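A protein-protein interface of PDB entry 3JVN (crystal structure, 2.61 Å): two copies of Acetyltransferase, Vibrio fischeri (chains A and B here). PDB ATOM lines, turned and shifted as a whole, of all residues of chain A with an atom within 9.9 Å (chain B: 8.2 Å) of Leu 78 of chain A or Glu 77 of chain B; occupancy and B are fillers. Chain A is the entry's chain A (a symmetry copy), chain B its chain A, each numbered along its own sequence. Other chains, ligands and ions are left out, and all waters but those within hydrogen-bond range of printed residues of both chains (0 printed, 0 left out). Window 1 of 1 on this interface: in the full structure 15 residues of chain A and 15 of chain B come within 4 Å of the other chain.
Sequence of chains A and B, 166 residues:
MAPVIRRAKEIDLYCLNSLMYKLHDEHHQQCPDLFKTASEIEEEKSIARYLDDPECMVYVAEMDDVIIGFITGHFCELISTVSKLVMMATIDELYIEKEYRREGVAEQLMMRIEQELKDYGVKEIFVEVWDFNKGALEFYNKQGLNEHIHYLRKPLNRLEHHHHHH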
ATOM      1  N   PHE A  75      40.757  25.536 -10.010  1.00  0.00           N
ATOM      2  CA  PHE A  75      39.354  25.752 -10.368  1.00  0.00           C
ATOM      3  C   PHE A  75      38.546  24.559  -9.859  1.00  0.00           C
ATOM      4  O   PHE A  75      39.055  23.431  -9.780  1.00  0.00           O
ATOM      5  CB  PHE A  75      39.169  25.857 -11.897  1.00  0.00           C
ATOM      6  CG  PHE A  75      39.692  27.136 -12.494  1.00  0.00           C
ATOM      7  CD1 PHE A  75      39.239  28.370 -12.026  1.00  0.00           C
ATOM      8  CD2 PHE A  75      40.644  27.105 -13.520  1.00  0.00           C
ATOM      9  CE1 PHE A  75      39.712  29.567 -12.562  1.00  0.00           C
ATOM     10  CE2 PHE A  75      41.135  28.291 -14.075  1.00  0.00           C
ATOM     11  CZ  PHE A  75      40.666  29.536 -13.588  1.00  0.00           C
ATOM     12  N   CYS A  76      37.296  24.809  -9.488  1.00  0.00           N
ATOM     13  CA  CYS A  76      36.423  23.739  -9.029  1.00  0.00           C
ATOM     14  C   CYS A  76      34.996  24.054  -9.421  1.00  0.00           C
ATOM     15  O   CYS A  76      34.666  25.185  -9.779  1.00  0.00           O
ATOM     16  CB  CYS A  76      36.531  23.518  -7.519  1.00  0.00           C
ATOM     17  SG  CYS A  76      37.124  24.916  -6.565  1.00  0.00           S
ATOM     18  N   GLU A  77      34.149  23.038  -9.376  1.00  0.00           N
ATOM     19  CA  GLU A  77      32.766  23.213  -9.769  1.00  0.00           C
ATOM     20  C   GLU A  77      31.782  22.659  -8.772  1.00  0.00           C
ATOM     21  O   GLU A  77      31.875  21.498  -8.363  1.00  0.00           O
ATOM     22  CB  GLU A  77      32.510  22.522 -11.106  1.00  0.00           C
ATOM     23  CG  GLU A  77      32.961  23.255 -12.343  1.00  0.00           C
ATOM     24  CD  GLU A  77      32.584  22.479 -13.587  1.00  0.00           C
ATOM     25  OE1 GLU A  77      32.303  23.108 -14.633  1.00  0.00           O
ATOM     26  OE2 GLU A  77      32.568  21.231 -13.497  1.00  0.00           O
ATOM     27  N   LEU A  78      30.835  23.505  -8.391  1.00  0.00           N
ATOM     28  CA  LEU A  78      29.777  23.110  -7.489  1.00  0.00           C
ATOM     29  C   LEU A  78      28.770  22.411  -8.404  1.00  0.00           C
ATOM     30  O   LEU A  78      28.084  23.044  -9.210  1.00  0.00           O
ATOM     31  CB  LEU A  78      29.154  24.338  -6.843  1.00  0.00           C
ATOM     32  CG  LEU A  78      27.938  24.073  -5.961  1.00  0.00           C
ATOM     33  CD1 LEU A  78      28.380  23.351  -4.697  1.00  0.00           C
ATOM     34  CD2 LEU A  78      27.270  25.394  -5.613  1.00  0.00           C
ATOM     35  N   ILE A  79      28.725  21.091  -8.298  1.00  0.00           N
ATOM     36  CA  ILE A  79      27.845  20.265  -9.109  1.00  0.00           C
ATOM     37  C   ILE A  79      26.609  19.828  -8.337  1.00  0.00           C
ATOM     38  O   ILE A  79      26.687  19.401  -7.172  1.00  0.00           O
ATOM     39  CB  ILE A  79      28.611  19.029  -9.620  1.00  0.00           C
ATOM     40  CG1 ILE A  79      29.647  19.481 -10.658  1.00  0.00           C
ATOM     41  CG2 ILE A  79      27.651  17.999 -10.172  1.00  0.00           C
ATOM     42  CD1 ILE A  79      30.540  18.355 -11.177  1.00  0.00           C
ATOM     43  N   SER A  80      25.459  19.944  -8.987  1.00  0.00           N
ATOM     44  CA  SER A  80      24.212  19.541  -8.373  1.00  0.00           C
ATOM     45  C   SER A  80      23.430  18.680  -9.355  1.00  0.00           C
ATOM     46  O   SER A  80      23.877  18.410 -10.477  1.00  0.00           O
ATOM     47  CB  SER A  80      23.383  20.757  -7.987  1.00  0.00           C
ATOM     48  OG  SER A  80      23.082  21.568  -9.105  1.00  0.00           O
ATOM     49  N   THR A  81      22.267  18.230  -8.917  1.00  0.00           N
ATOM     50  CA  THR A  81      21.422  17.407  -9.755  1.00  0.00           C
ATOM     51  C   THR A  81      20.233  18.225 -10.258  1.00  0.00           C
ATOM     52  O   THR A  81      19.346  17.695 -10.930  1.00  0.00           O
ATOM     53  CB  THR A  81      20.893  16.207  -8.968  1.00  0.00           C
ATOM     54  OG1 THR A  81      20.142  16.677  -7.843  1.00  0.00           O
ATOM     55  CG2 THR A  81      22.033  15.349  -8.478  1.00  0.00           C
ATOM     56  N   VAL A  82      20.224  19.516  -9.945  1.00  0.00           N
ATOM     57  CA  VAL A  82      19.121  20.376 -10.352  1.00  0.00           C
ATOM     58  C   VAL A  82      19.554  21.731 -10.876  1.00  0.00           C
ATOM     59  O   VAL A  82      18.718  22.597 -11.119  1.00  0.00           O
ATOM     60  CB  VAL A  82      18.160  20.625  -9.185  1.00  0.00           C
ATOM     61  CG1 VAL A  82      17.658  19.299  -8.642  1.00  0.00           C
ATOM     62  CG2 VAL A  82      18.863  21.420  -8.096  1.00  0.00           C
ATOM     63  N   SER A  83      20.855  21.927 -11.039  1.00  0.00           N
ATOM     64  CA  SER A  83      21.355  23.198 -11.539  1.00  0.00           C
ATOM     65  C   SER A  83      22.633  22.990 -12.308  1.00  0.00           C
ATOM     66  O   SER A  83      23.388  22.050 -12.049  1.00  0.00           O
ATOM     67  CB  SER A  83      21.635  24.167 -10.387  1.00  0.00           C
ATOM     68  OG  SER A  83      20.450  24.525  -9.699  1.00  0.00           O
ATOM     69  N   LYS A  84      22.870  23.877 -13.259  1.00  0.00           N
ATOM     70  CA  LYS A  84      24.080  23.812 -14.047  1.00  0.00           C
ATOM     71  C   LYS A  84      25.254  24.077 -13.102  1.00  0.00           C
ATOM     72  O   LYS A  84      25.111  24.758 -12.088  1.00  0.00           O
ATOM     73  CB  LYS A  84      24.037  24.857 -15.172  1.00  0.00           C
ATOM     74  CG  LYS A  84      23.973  24.257 -16.578  1.00  0.00           C
ATOM     75  CD  LYS A  84      22.556  23.851 -16.993  1.00  0.00           C
ATOM     76  CE  LYS A  84      22.556  22.568 -17.845  1.00  0.00           C
ATOM     77  NZ  LYS A  84      23.524  22.585 -18.996  1.00  0.00           N
ATOM     78  N   LEU A  85      26.410  23.527 -13.440  1.00  0.00           N
ATOM     79  CA  LEU A  85      27.602  23.694 -12.632  1.00  0.00           C
ATOM     80  C   LEU A  85      27.956  25.182 -12.477  1.00  0.00           C
ATOM     81  O   LEU A  85      27.827  25.958 -13.422  1.00  0.00           O
ATOM     82  CB  LEU A  85      28.758  22.926 -13.280  1.00  0.00           C
ATOM     83  CG  LEU A  85      28.387  21.570 -13.880  1.00  0.00           C
ATOM     84  CD1 LEU A  85      27.541  20.784 -12.883  1.00  0.00           C
ATOM     85  CD2 LEU A  85      27.614  21.768 -15.175  1.00  0.00           C
ATOM     86  N   VAL A  86      28.388  25.568 -11.276  1.00  0.00           N
ATOM     87  CA  VAL A  86      28.770  26.946 -10.977  1.00  0.00           C
ATOM     88  C   VAL A  86      30.280  26.968 -10.901  1.00  0.00           C
ATOM     89  O   VAL A  86      30.878  26.156 -10.203  1.00  0.00           O
ATOM     90  CB  VAL A  86      28.216  27.395  -9.605  1.00  0.00           C
ATOM     91  CG1 VAL A  86      28.429  28.890  -9.412  1.00  0.00           C
ATOM     92  CG2 VAL A  86      26.754  27.034  -9.485  1.00  0.00           C
ATOM     93  N   MET A  87      30.910  27.890 -11.609  1.00  0.00           N
ATOM     94  CA  MET A  87      32.358  27.940 -11.577  1.00  0.00           C
ATOM     95  C   MET A  87      32.886  28.607 -10.313  1.00  0.00           C
ATOM     96  O   MET A  87      32.530  29.742  -9.992  1.00  0.00           O
ATOM     97  CB  MET A  87      32.900  28.673 -12.801  1.00  0.00           C
ATOM     98  CG  MET A  87      34.434  28.819 -12.807  1.00  0.00           C
ATOM     99  SD  MET A  87      35.411  27.157 -13.099  1.00  0.00           S
ATOM    100  CE  MET A  87      36.525  27.739 -14.567  1.00  0.00           C
ATOM    101  N   MET A  88      33.741  27.889  -9.597  1.00  0.00           N
ATOM    102  CA  MET A  88      34.344  28.412  -8.382  1.00  0.00           C
ATOM    103  C   MET A  88      35.801  28.009  -8.371  1.00  0.00           C
ATOM    104  O   MET A  88      36.263  27.283  -9.252  1.00  0.00           O
ATOM    105  CB  MET A  88      33.652  27.844  -7.145  1.00  0.00           C
ATOM    106  CG  MET A  88      32.152  28.009  -7.131  1.00  0.00           C
ATOM    107  SD  MET A  88      31.437  27.488  -5.420  1.00  0.00           S
ATOM    108  CE  MET A  88      29.602  28.023  -5.692  1.00  0.00           C
ATOM    109  N   ALA A  89      36.524  28.476  -7.366  1.00  0.00           N
ATOM    110  CA  ALA A  89      37.929  28.152  -7.260  1.00  0.00           C
ATOM    111  C   ALA A  89      38.396  28.129  -5.816  1.00  0.00           C
ATOM    112  O   ALA A  89      37.662  28.507  -4.901  1.00  0.00           O
ATOM    113  CB  ALA A  89      38.782  29.148  -8.076  1.00  0.00           C
ATOM    114  N   THR A  90      39.640  27.699  -5.626  1.00  0.00           N
ATOM    115  CA  THR A  90      40.235  27.610  -4.297  1.00  0.00           C
ATOM    116  C   THR A  90      41.712  28.021  -4.322  1.00  0.00           C
ATOM    117  O   THR A  90      42.474  27.576  -5.178  1.00  0.00           O
ATOM    118  CB  THR A  90      40.153  26.156  -3.742  1.00  0.00           C
ATOM    119  OG1 THR A  90      38.831  25.640  -3.935  1.00  0.00           O
ATOM    120  CG2 THR A  90      40.481  26.128  -2.256  1.00  0.00           C
ATOM    121  N   LYS A 123      32.555  32.451  -9.463  1.00  0.00           N
ATOM    122  CA  LYS A 123      31.504  33.003  -8.626  1.00  0.00           C
ATOM    123  C   LYS A 123      31.924  33.064  -7.170  1.00  0.00           C
ATOM    124  O   LYS A 123      31.718  34.082  -6.511  1.00  0.00           O
ATOM    125  CB  LYS A 123      30.238  32.166  -8.770  1.00  0.00           C
ATOM    126  CG  LYS A 123      29.829  31.912 -10.228  1.00  0.00           C
ATOM    127  CD  LYS A 123      29.775  33.201 -11.031  1.00  0.00           C
ATOM    128  CE  LYS A 123      29.229  32.945 -12.420  1.00  0.00           C
ATOM    129  NZ  LYS A 123      29.282  34.161 -13.287  1.00  0.00           N
ATOM    130  N   GLU A 124      32.514  31.975  -6.672  1.00  0.00           N
ATOM    131  CA  GLU A 124      32.973  31.905  -5.285  1.00  0.00           C
ATOM    132  C   GLU A 124      34.449  31.518  -5.161  1.00  0.00           C
ATOM    133  O   GLU A 124      34.960  30.736  -5.958  1.00  0.00           O
ATOM    134  CB  GLU A 124      32.122  30.903  -4.496  1.00  0.00           C
ATOM    135  CG  GLU A 124      30.650  31.287  -4.361  1.00  0.00           C
ATOM    136  CD  GLU A 124      30.458  32.722  -3.900  1.00  0.00           C
ATOM    137  OE1 GLU A 124      31.167  33.128  -2.951  1.00  0.00           O
ATOM    138  OE2 GLU A 124      29.594  33.432  -4.473  1.00  0.00           O
ATOM    139  N   PHE A 126      37.394  30.232  -2.234  1.00  0.00           N
ATOM    140  CA  PHE A 126      37.726  29.730  -0.901  1.00  0.00           C
ATOM    141  C   PHE A 126      39.231  29.764  -0.693  1.00  0.00           C
ATOM    142  O   PHE A 126      39.966  29.099  -1.417  1.00  0.00           O
ATOM    143  CB  PHE A 126      37.242  28.288  -0.755  1.00  0.00           C
ATOM    144  CG  PHE A 126      35.778  28.115  -0.989  1.00  0.00           C
ATOM    145  CD1 PHE A 126      34.861  28.505  -0.024  1.00  0.00           C
ATOM    146  CD2 PHE A 126      35.314  27.585  -2.191  1.00  0.00           C
ATOM    147  CE1 PHE A 126      33.502  28.370  -0.255  1.00  0.00           C
ATOM    148  CE2 PHE A 126      33.959  27.444  -2.431  1.00  0.00           C
ATOM    149  CZ  PHE A 126      33.047  27.838  -1.465  1.00  0.00           C
ATOM    150  N   GLU B  55      18.631  14.201  -3.843  1.00  0.00           N
ATOM    151  CA  GLU B  55      19.529  15.230  -3.310  1.00  0.00           C
ATOM    152  C   GLU B  55      18.762  16.503  -2.928  1.00  0.00           C
ATOM    153  O   GLU B  55      19.374  17.484  -2.483  1.00  0.00           O
ATOM    154  CB  GLU B  55      20.597  15.602  -4.348  1.00  0.00           C
ATOM    155  CG  GLU B  55      21.508  14.467  -4.826  1.00  0.00           C
ATOM    156  CD  GLU B  55      22.158  13.675  -3.689  1.00  0.00           C
ATOM    157  OE1 GLU B  55      22.231  14.186  -2.554  1.00  0.00           O
ATOM    158  OE2 GLU B  55      22.599  12.535  -3.938  1.00  0.00           O
ATOM    159  N   HIS B  74      18.842  22.115  -1.769  1.00  0.00           N
ATOM    160  CA  HIS B  74      19.449  20.926  -2.381  1.00  0.00           C
ATOM    161  C   HIS B  74      20.926  20.724  -2.053  1.00  0.00           C
ATOM    162  O   HIS B  74      21.659  21.689  -1.883  1.00  0.00           O
ATOM    163  CB  HIS B  74      19.278  20.944  -3.914  1.00  0.00           C
ATOM    164  CG  HIS B  74      20.160  21.926  -4.634  1.00  0.00           C
ATOM    165  ND1 HIS B  74      19.915  23.283  -4.646  1.00  0.00           N
ATOM    166  CD2 HIS B  74      21.249  21.737  -5.419  1.00  0.00           C
ATOM    167  CE1 HIS B  74      20.811  23.886  -5.407  1.00  0.00           C
ATOM    168  NE2 HIS B  74      21.633  22.972  -5.890  1.00  0.00           N
ATOM    169  N   PHE B  75      21.348  19.463  -1.953  1.00  0.00           N
ATOM    170  CA  PHE B  75      22.749  19.140  -1.679  1.00  0.00           C
ATOM    171  C   PHE B  75      23.543  19.343  -2.970  1.00  0.00           C
ATOM    172  O   PHE B  75      23.015  19.167  -4.078  1.00  0.00           O
ATOM    173  CB  PHE B  75      22.914  17.675  -1.224  1.00  0.00           C
ATOM    174  CG  PHE B  75      22.406  17.401   0.165  1.00  0.00           C
ATOM    175  CD1 PHE B  75      22.888  18.135   1.250  1.00  0.00           C
ATOM    176  CD2 PHE B  75      21.439  16.414   0.388  1.00  0.00           C
ATOM    177  CE1 PHE B  75      22.428  17.901   2.546  1.00  0.00           C
ATOM    178  CE2 PHE B  75      20.962  16.159   1.678  1.00  0.00           C
ATOM    179  CZ  PHE B  75      21.460  16.913   2.768  1.00  0.00           C
ATOM    180  N   CYS B  76      24.802  19.740  -2.831  1.00  0.00           N
ATOM    181  CA  CYS B  76      25.662  19.921  -3.991  1.00  0.00           C
ATOM    182  C   CYS B  76      27.089  19.588  -3.614  1.00  0.00           C
ATOM    183  O   CYS B  76      27.434  19.497  -2.435  1.00  0.00           O
ATOM    184  CB  CYS B  76      25.572  21.340  -4.555  1.00  0.00           C
ATOM    185  SG  CYS B  76      25.017  22.604  -3.410  1.00  0.00           S
ATOM    186  N   GLU B  77      27.918  19.380  -4.624  1.00  0.00           N
ATOM    187  CA  GLU B  77      29.298  19.013  -4.382  1.00  0.00           C
ATOM    188  C   GLU B  77      30.286  19.837  -5.167  1.00  0.00           C
ATOM    189  O   GLU B  77      30.178  19.966  -6.390  1.00  0.00           O
ATOM    190  CB  GLU B  77      29.523  17.548  -4.746  1.00  0.00           C
ATOM    191  CG  GLU B  77      29.068  16.524  -3.739  1.00  0.00           C
ATOM    192  CD  GLU B  77      29.413  15.127  -4.209  1.00  0.00           C
ATOM    193  OE1 GLU B  77      29.689  14.251  -3.358  1.00  0.00           O
ATOM    194  OE2 GLU B  77      29.408  14.924  -5.444  1.00  0.00           O
ATOM    195  N   LEU B  78      31.253  20.387  -4.446  1.00  0.00           N
ATOM    196  CA  LEU B  78      32.317  21.153  -5.055  1.00  0.00           C
ATOM    197  C   LEU B  78      33.298  20.082  -5.536  1.00  0.00           C
ATOM    198  O   LEU B  78      33.984  19.434  -4.743  1.00  0.00           O
ATOM    199  CB  LEU B  78      32.972  22.055  -4.020  1.00  0.00           C
ATOM    200  CG  LEU B  78      34.194  22.830  -4.501  1.00  0.00           C
ATOM    201  CD1 LEU B  78      33.758  23.898  -5.491  1.00  0.00           C
ATOM    202  CD2 LEU B  78      34.891  23.463  -3.307  1.00  0.00           C
ATOM    203  N   ILE B  79      33.321  19.878  -6.845  1.00  0.00           N
ATOM    204  CA  ILE B  79      34.174  18.881  -7.472  1.00  0.00           C
ATOM    205  C   ILE B  79      35.413  19.508  -8.094  1.00  0.00           C
ATOM    206  O   ILE B  79      35.344  20.543  -8.780  1.00  0.00           O
ATOM    207  CB  ILE B  79      33.379  18.111  -8.544  1.00  0.00           C
ATOM    208  CG1 ILE B  79      32.336  17.225  -7.848  1.00  0.00           C
ATOM    209  CG2 ILE B  79      34.312  17.316  -9.431  1.00  0.00           C
ATOM    210  CD1 ILE B  79      31.416  16.475  -8.809  1.00  0.00           C
ATOM    211  N   SER B  80      36.555  18.882  -7.846  1.00  0.00           N
ATOM    212  CA  SER B  80      37.804  19.362  -8.400  1.00  0.00           C
ATOM    213  C   SER B  80      38.556  18.194  -9.019  1.00  0.00           C
ATOM    214  O   SER B  80      38.088  17.048  -9.014  1.00  0.00           O
ATOM    215  CB  SER B  80      38.660  20.006  -7.318  1.00  0.00           C
ATOM    216  OG  SER B  80      38.959  19.102  -6.274  1.00  0.00           O
ATOM    217  N   LYS B  84      39.154  15.596  -3.064  1.00  0.00           N
ATOM    218  CA  LYS B  84      37.932  14.836  -2.927  1.00  0.00           C
ATOM    219  C   LYS B  84      36.777  15.838  -2.872  1.00  0.00           C
ATOM    220  O   LYS B  84      36.946  16.980  -2.448  1.00  0.00           O
ATOM    221  CB  LYS B  84      37.978  13.985  -1.650  1.00  0.00           C
ATOM    222  CG  LYS B  84      38.010  12.476  -1.907  1.00  0.00           C
ATOM    223  CD  LYS B  84      39.415  11.953  -2.225  1.00  0.00           C
ATOM    224  CE  LYS B  84      39.379  10.827  -3.274  1.00  0.00           C
ATOM    225  NZ  LYS B  84      38.395   9.728  -2.976  1.00  0.00           N
ATOM    226  N   LEU B  85      35.606  15.402  -3.312  1.00  0.00           N
ATOM    227  CA  LEU B  85      34.428  16.249  -3.321  1.00  0.00           C
ATOM    228  C   LEU B  85      34.103  16.751  -1.905  1.00  0.00           C
ATOM    229  O   LEU B  85      34.233  16.011  -0.932  1.00  0.00           O
ATOM    230  CB  LEU B  85      33.250  15.460  -3.900  1.00  0.00           C
ATOM    231  CG  LEU B  85      33.588  14.555  -5.085  1.00  0.00           C
ATOM    232  CD1 LEU B  85      34.434  15.327  -6.093  1.00  0.00           C
ATOM    233  CD2 LEU B  85      34.345  13.328  -4.602  1.00  0.00           C
ATOM    234  N   VAL B  86      33.697  18.017  -1.803  1.00  0.00           N
ATOM    235  CA  VAL B  86      33.343  18.635  -0.527  1.00  0.00           C
ATOM    236  C   VAL B  86      31.835  18.741  -0.503  1.00  0.00           C
ATOM    237  O   VAL B  86      31.232  19.242  -1.446  1.00  0.00           O
ATOM    238  CB  VAL B  86      33.925  20.063  -0.418  1.00  0.00           C
ATOM    239  CG1 VAL B  86      33.742  20.603   0.994  1.00  0.00           C
ATOM    240  CG2 VAL B  86      35.381  20.070  -0.818  1.00  0.00           C
ATOM    241  N   MET B  87      31.212  18.278   0.568  1.00  0.00           N
ATOM    242  CA  MET B  87      29.766  18.347   0.629  1.00  0.00           C
ATOM    243  C   MET B  87      29.268  19.741   0.992  1.00  0.00           C
ATOM    244  O   MET B  87      29.648  20.311   2.016  1.00  0.00           O
ATOM    245  CB  MET B  87      29.220  17.337   1.636  1.00  0.00           C
ATOM    246  CG  MET B  87      27.689  17.394   1.801  1.00  0.00           C
ATOM    247  SD  MET B  87      26.678  16.741   0.266  1.00  0.00           S
ATOM    248  CE  MET B  87      25.553  15.469   1.190  1.00  0.00           C
ATOM    249  N   MET B  88      28.410  20.285   0.139  1.00  0.00           N
ATOM    250  CA  MET B  88      27.834  21.599   0.373  1.00  0.00           C
ATOM    251  C   MET B  88      26.371  21.543   0.000  1.00  0.00           C
ATOM    252  O   MET B  88      25.883  20.526  -0.495  1.00  0.00           O
ATOM    253  CB  MET B  88      28.533  22.658  -0.477  1.00  0.00           C
ATOM    254  CG  MET B  88      30.036  22.683  -0.341  1.00  0.00           C
ATOM    255  SD  MET B  88      30.766  24.213  -1.257  1.00  0.00           S
ATOM    256  CE  MET B  88      32.606  24.040  -0.699  1.00  0.00           C
ATOM    257  N   ALA B  89      25.670  22.642   0.230  1.00  0.00           N
ATOM    258  CA  ALA B  89      24.261  22.695  -0.090  1.00  0.00           C
ATOM    259  C   ALA B  89      23.814  24.102  -0.442  1.00  0.00           C
ATOM    260  O   ALA B  89      24.568  25.066  -0.297  1.00  0.00           O
ATOM    261  CB  ALA B  89      23.415  22.149   1.081  1.00  0.00           C
ATOM    262  N   THR B  90      22.566  24.209  -0.887  1.00  0.00           N
ATOM    263  CA  THR B  90      21.989  25.492  -1.274  1.00  0.00           C
ATOM    264  C   THR B  90      20.519  25.590  -0.847  1.00  0.00           C
ATOM    265  O   THR B  90      19.737  24.667  -1.070  1.00  0.00           O
ATOM    266  CB  THR B  90      22.052  25.692  -2.818  1.00  0.00           C
ATOM    267  OG1 THR B  90      23.362  25.360  -3.294  1.00  0.00           O
ATOM    268  CG2 THR B  90      21.745  27.136  -3.187  1.00  0.00           C
ATOM    269  N   GLU B 124      29.752  24.058   3.414  1.00  0.00           N
ATOM    270  CA  GLU B 124      29.312  25.399   3.029  1.00  0.00           C
ATOM    271  C   GLU B 124      27.830  25.456   2.645  1.00  0.00           C
ATOM    272  O   GLU B 124      27.294  24.508   2.077  1.00  0.00           O
ATOM    273  CB  GLU B 124      30.156  25.918   1.859  1.00  0.00           C
ATOM    274  CG  GLU B 124      31.636  26.112   2.180  1.00  0.00           C
ATOM    275  CD  GLU B 124      31.860  26.890   3.465  1.00  0.00           C
ATOM    276  OE1 GLU B 124      31.172  27.920   3.650  1.00  0.00           O
ATOM    277  OE2 GLU B 124      32.729  26.483   4.277  1.00  0.00           O
ATOM    278  N   PHE B 126      24.905  28.057   0.755  1.00  0.00           N
ATOM    279  CA  PHE B 126      24.583  29.242  -0.039  1.00  0.00           C
ATOM    280  C   PHE B 126      23.082  29.479  -0.033  1.00  0.00           C
ATOM    281  O   PHE B 126      22.324  28.633  -0.500  1.00  0.00           O
ATOM    282  CB  PHE B 126      25.043  29.040  -1.482  1.00  0.00           C
ATOM    283  CG  PHE B 126      26.500  28.746  -1.616  1.00  0.00           C
ATOM    284  CD1 PHE B 126      27.438  29.758  -1.475  1.00  0.00           C
ATOM    285  CD2 PHE B 126      26.937  27.446  -1.859  1.00  0.00           C
ATOM    286  CE1 PHE B 126      28.791  29.478  -1.572  1.00  0.00           C
ATOM    287  CE2 PHE B 126      28.286  27.154  -1.959  1.00  0.00           C
ATOM    288  CZ  PHE B 126      29.218  28.169  -1.814  1.00  0.00           C
ATOM    289  N   GLU B 128      19.833  31.322  -1.392  1.00  0.00           N
ATOM    290  CA  GLU B 128      19.363  31.981  -2.609  1.00  0.00           C
ATOM    291  C   GLU B 128      18.014  32.664  -2.398  1.00  0.00           C
ATOM    292  O   GLU B 128      17.455  33.220  -3.337  1.00  0.00           O
ATOM    293  CB  GLU B 128      19.201  30.956  -3.738  1.00  0.00           C
ATOM    294  CG  GLU B 128      20.348  29.982  -3.929  1.00  0.00           C
ATOM    295  CD  GLU B 128      21.590  30.624  -4.511  1.00  0.00           C
ATOM    296  OE1 GLU B 128      22.150  31.524  -3.852  1.00  0.00           O
ATOM    297  OE2 GLU B 128      22.008  30.232  -5.624  1.00  0.00           O
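The backbone NH of Ala 89 of chain A lies within hydrogen-bond range of the backbone carbonyl oxygen of Glu 124 of chain A.
The backbone carbonyl oxygen (O) of Val 86 of chain B sits at hydrogen-bond distance from the backbone NH (N) of Leu 78 of chain B, at 3.2 Å.
The side-chain hydroxyl (OG1) of Thr 90 of chain A is in hydrogen-bond range of the side-chain sulfur (SG) of Cys 76 of chain A (3.2 Å).
The side-chain sulfur (SG) of Cys 76 of chain A lies close to the backbone NH (N) of Ala 89 of chain A (3.7 Å).
OG of Ser 80 of chain A is in hydrogen-bond range of N of Ser 83 of chain A (3.0 Å).
N of His 74 of chain B lies within hydrogen-bond range of O of Thr 90 of chain B (2.8 Å).
Among the printed residues, merely in contact across the chains: Cys 76 of chain A with Leu 78 of chain B (3.5 Å), Cys 76 of chain A with Ile 79 of chain B (3.4 Å), Glu 77 of chain A with Leu 78 of chain B (3.4 Å), Leu 78 of chain A with Cys 76 of chain B (3.5 Å), Leu 78 of chain A with Glu 77 of chain B (3.4 Å), Ile 79 of chain A with Cys 76 of chain B (3.4 Å), Ile 79 of chain A with Ile 79 of chain B (3.1 Å), Ser 80 of chain A with His 74 of chain B (3.5 Å), Thr 81 of chain A with Glu 55 of chain B (3.7 Å), Val 82 of chain A with His 74 of chain B (3.6 Å), Met 88 of chain A with Phe 126 of chain B (3.9 Å), Glu 124 of chain A with Phe 126 of chain B (3.8 Å), Phe 126 of chain A with Met 88 of chain B (3.9 Å), Phe 126 of chain A with Glu 124 of chain B (3.8 Å) and Phe 126 of chain A with Phe 126 of chain B (3.9 Å).
Glu 77 of chain B touches its own counterpart, Glu 77 of chain A.
Ile 79 of chain A touches its own counterpart, Ile 79 of chain B.
Glu 124 of chain A touches Phe 126 of chain B, and with the chains exchanged Phe 126 of chain A touches Glu 124 of chain B.
Phe 126 of chain B touches its own counterpart, Phe 126 of chain A.
Of the 18 pairs that touch across the chains among the printed residues, 15 have their exchanged pair printed and touching as well.
Leu 78 of chain A touches two residues of chain B.
Glu 77 of chain B touches three residues of chain A.
Cys 76 of chain B touches two residues of chain A.
Of chain A, only Cys 76 (3.4 Å), Glu 77 (2.6 Å) and Ile 79 (3.1 Å) come within 4 Å of Ile 79 of chain B.
Printed residues of chain B within 4 Å of Glu 77 of chain A: Glu 77, Leu 78 and Ile 79.
Printed residues of chain B within 4 Å of Met 88 of chain A: Phe 126 (3.9 Å).
Of the 19 printed residues of chain A, 10 touch a printed residue of chain B.
Printed residues of chain B that touch a printed residue of chain A: Glu 55, His 74, Cys 76, Glu 77, Leu 78, Ile 79, Met 88, Glu 124 and Phe 126.
Hydrophobic or aromatic side chains of chain B within 4 Å of the printed part of chain A: His 74, Leu 78, Ile 79, Met 88 and Phe 126.
The backbone carbonyl oxygen (O) of Glu 77 of chain B sits at hydrogen-bond distance from the backbone NH (N) of Ile 79 of chain A, 2.6 Å away.
O of Glu 77 of chain B lies close to O of Glu 77 of chain A (3.0 Å).
N of Ile 79 of chain B sits at hydrogen-bond distance from O of Glu 77 of chain A (2.6 Å).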
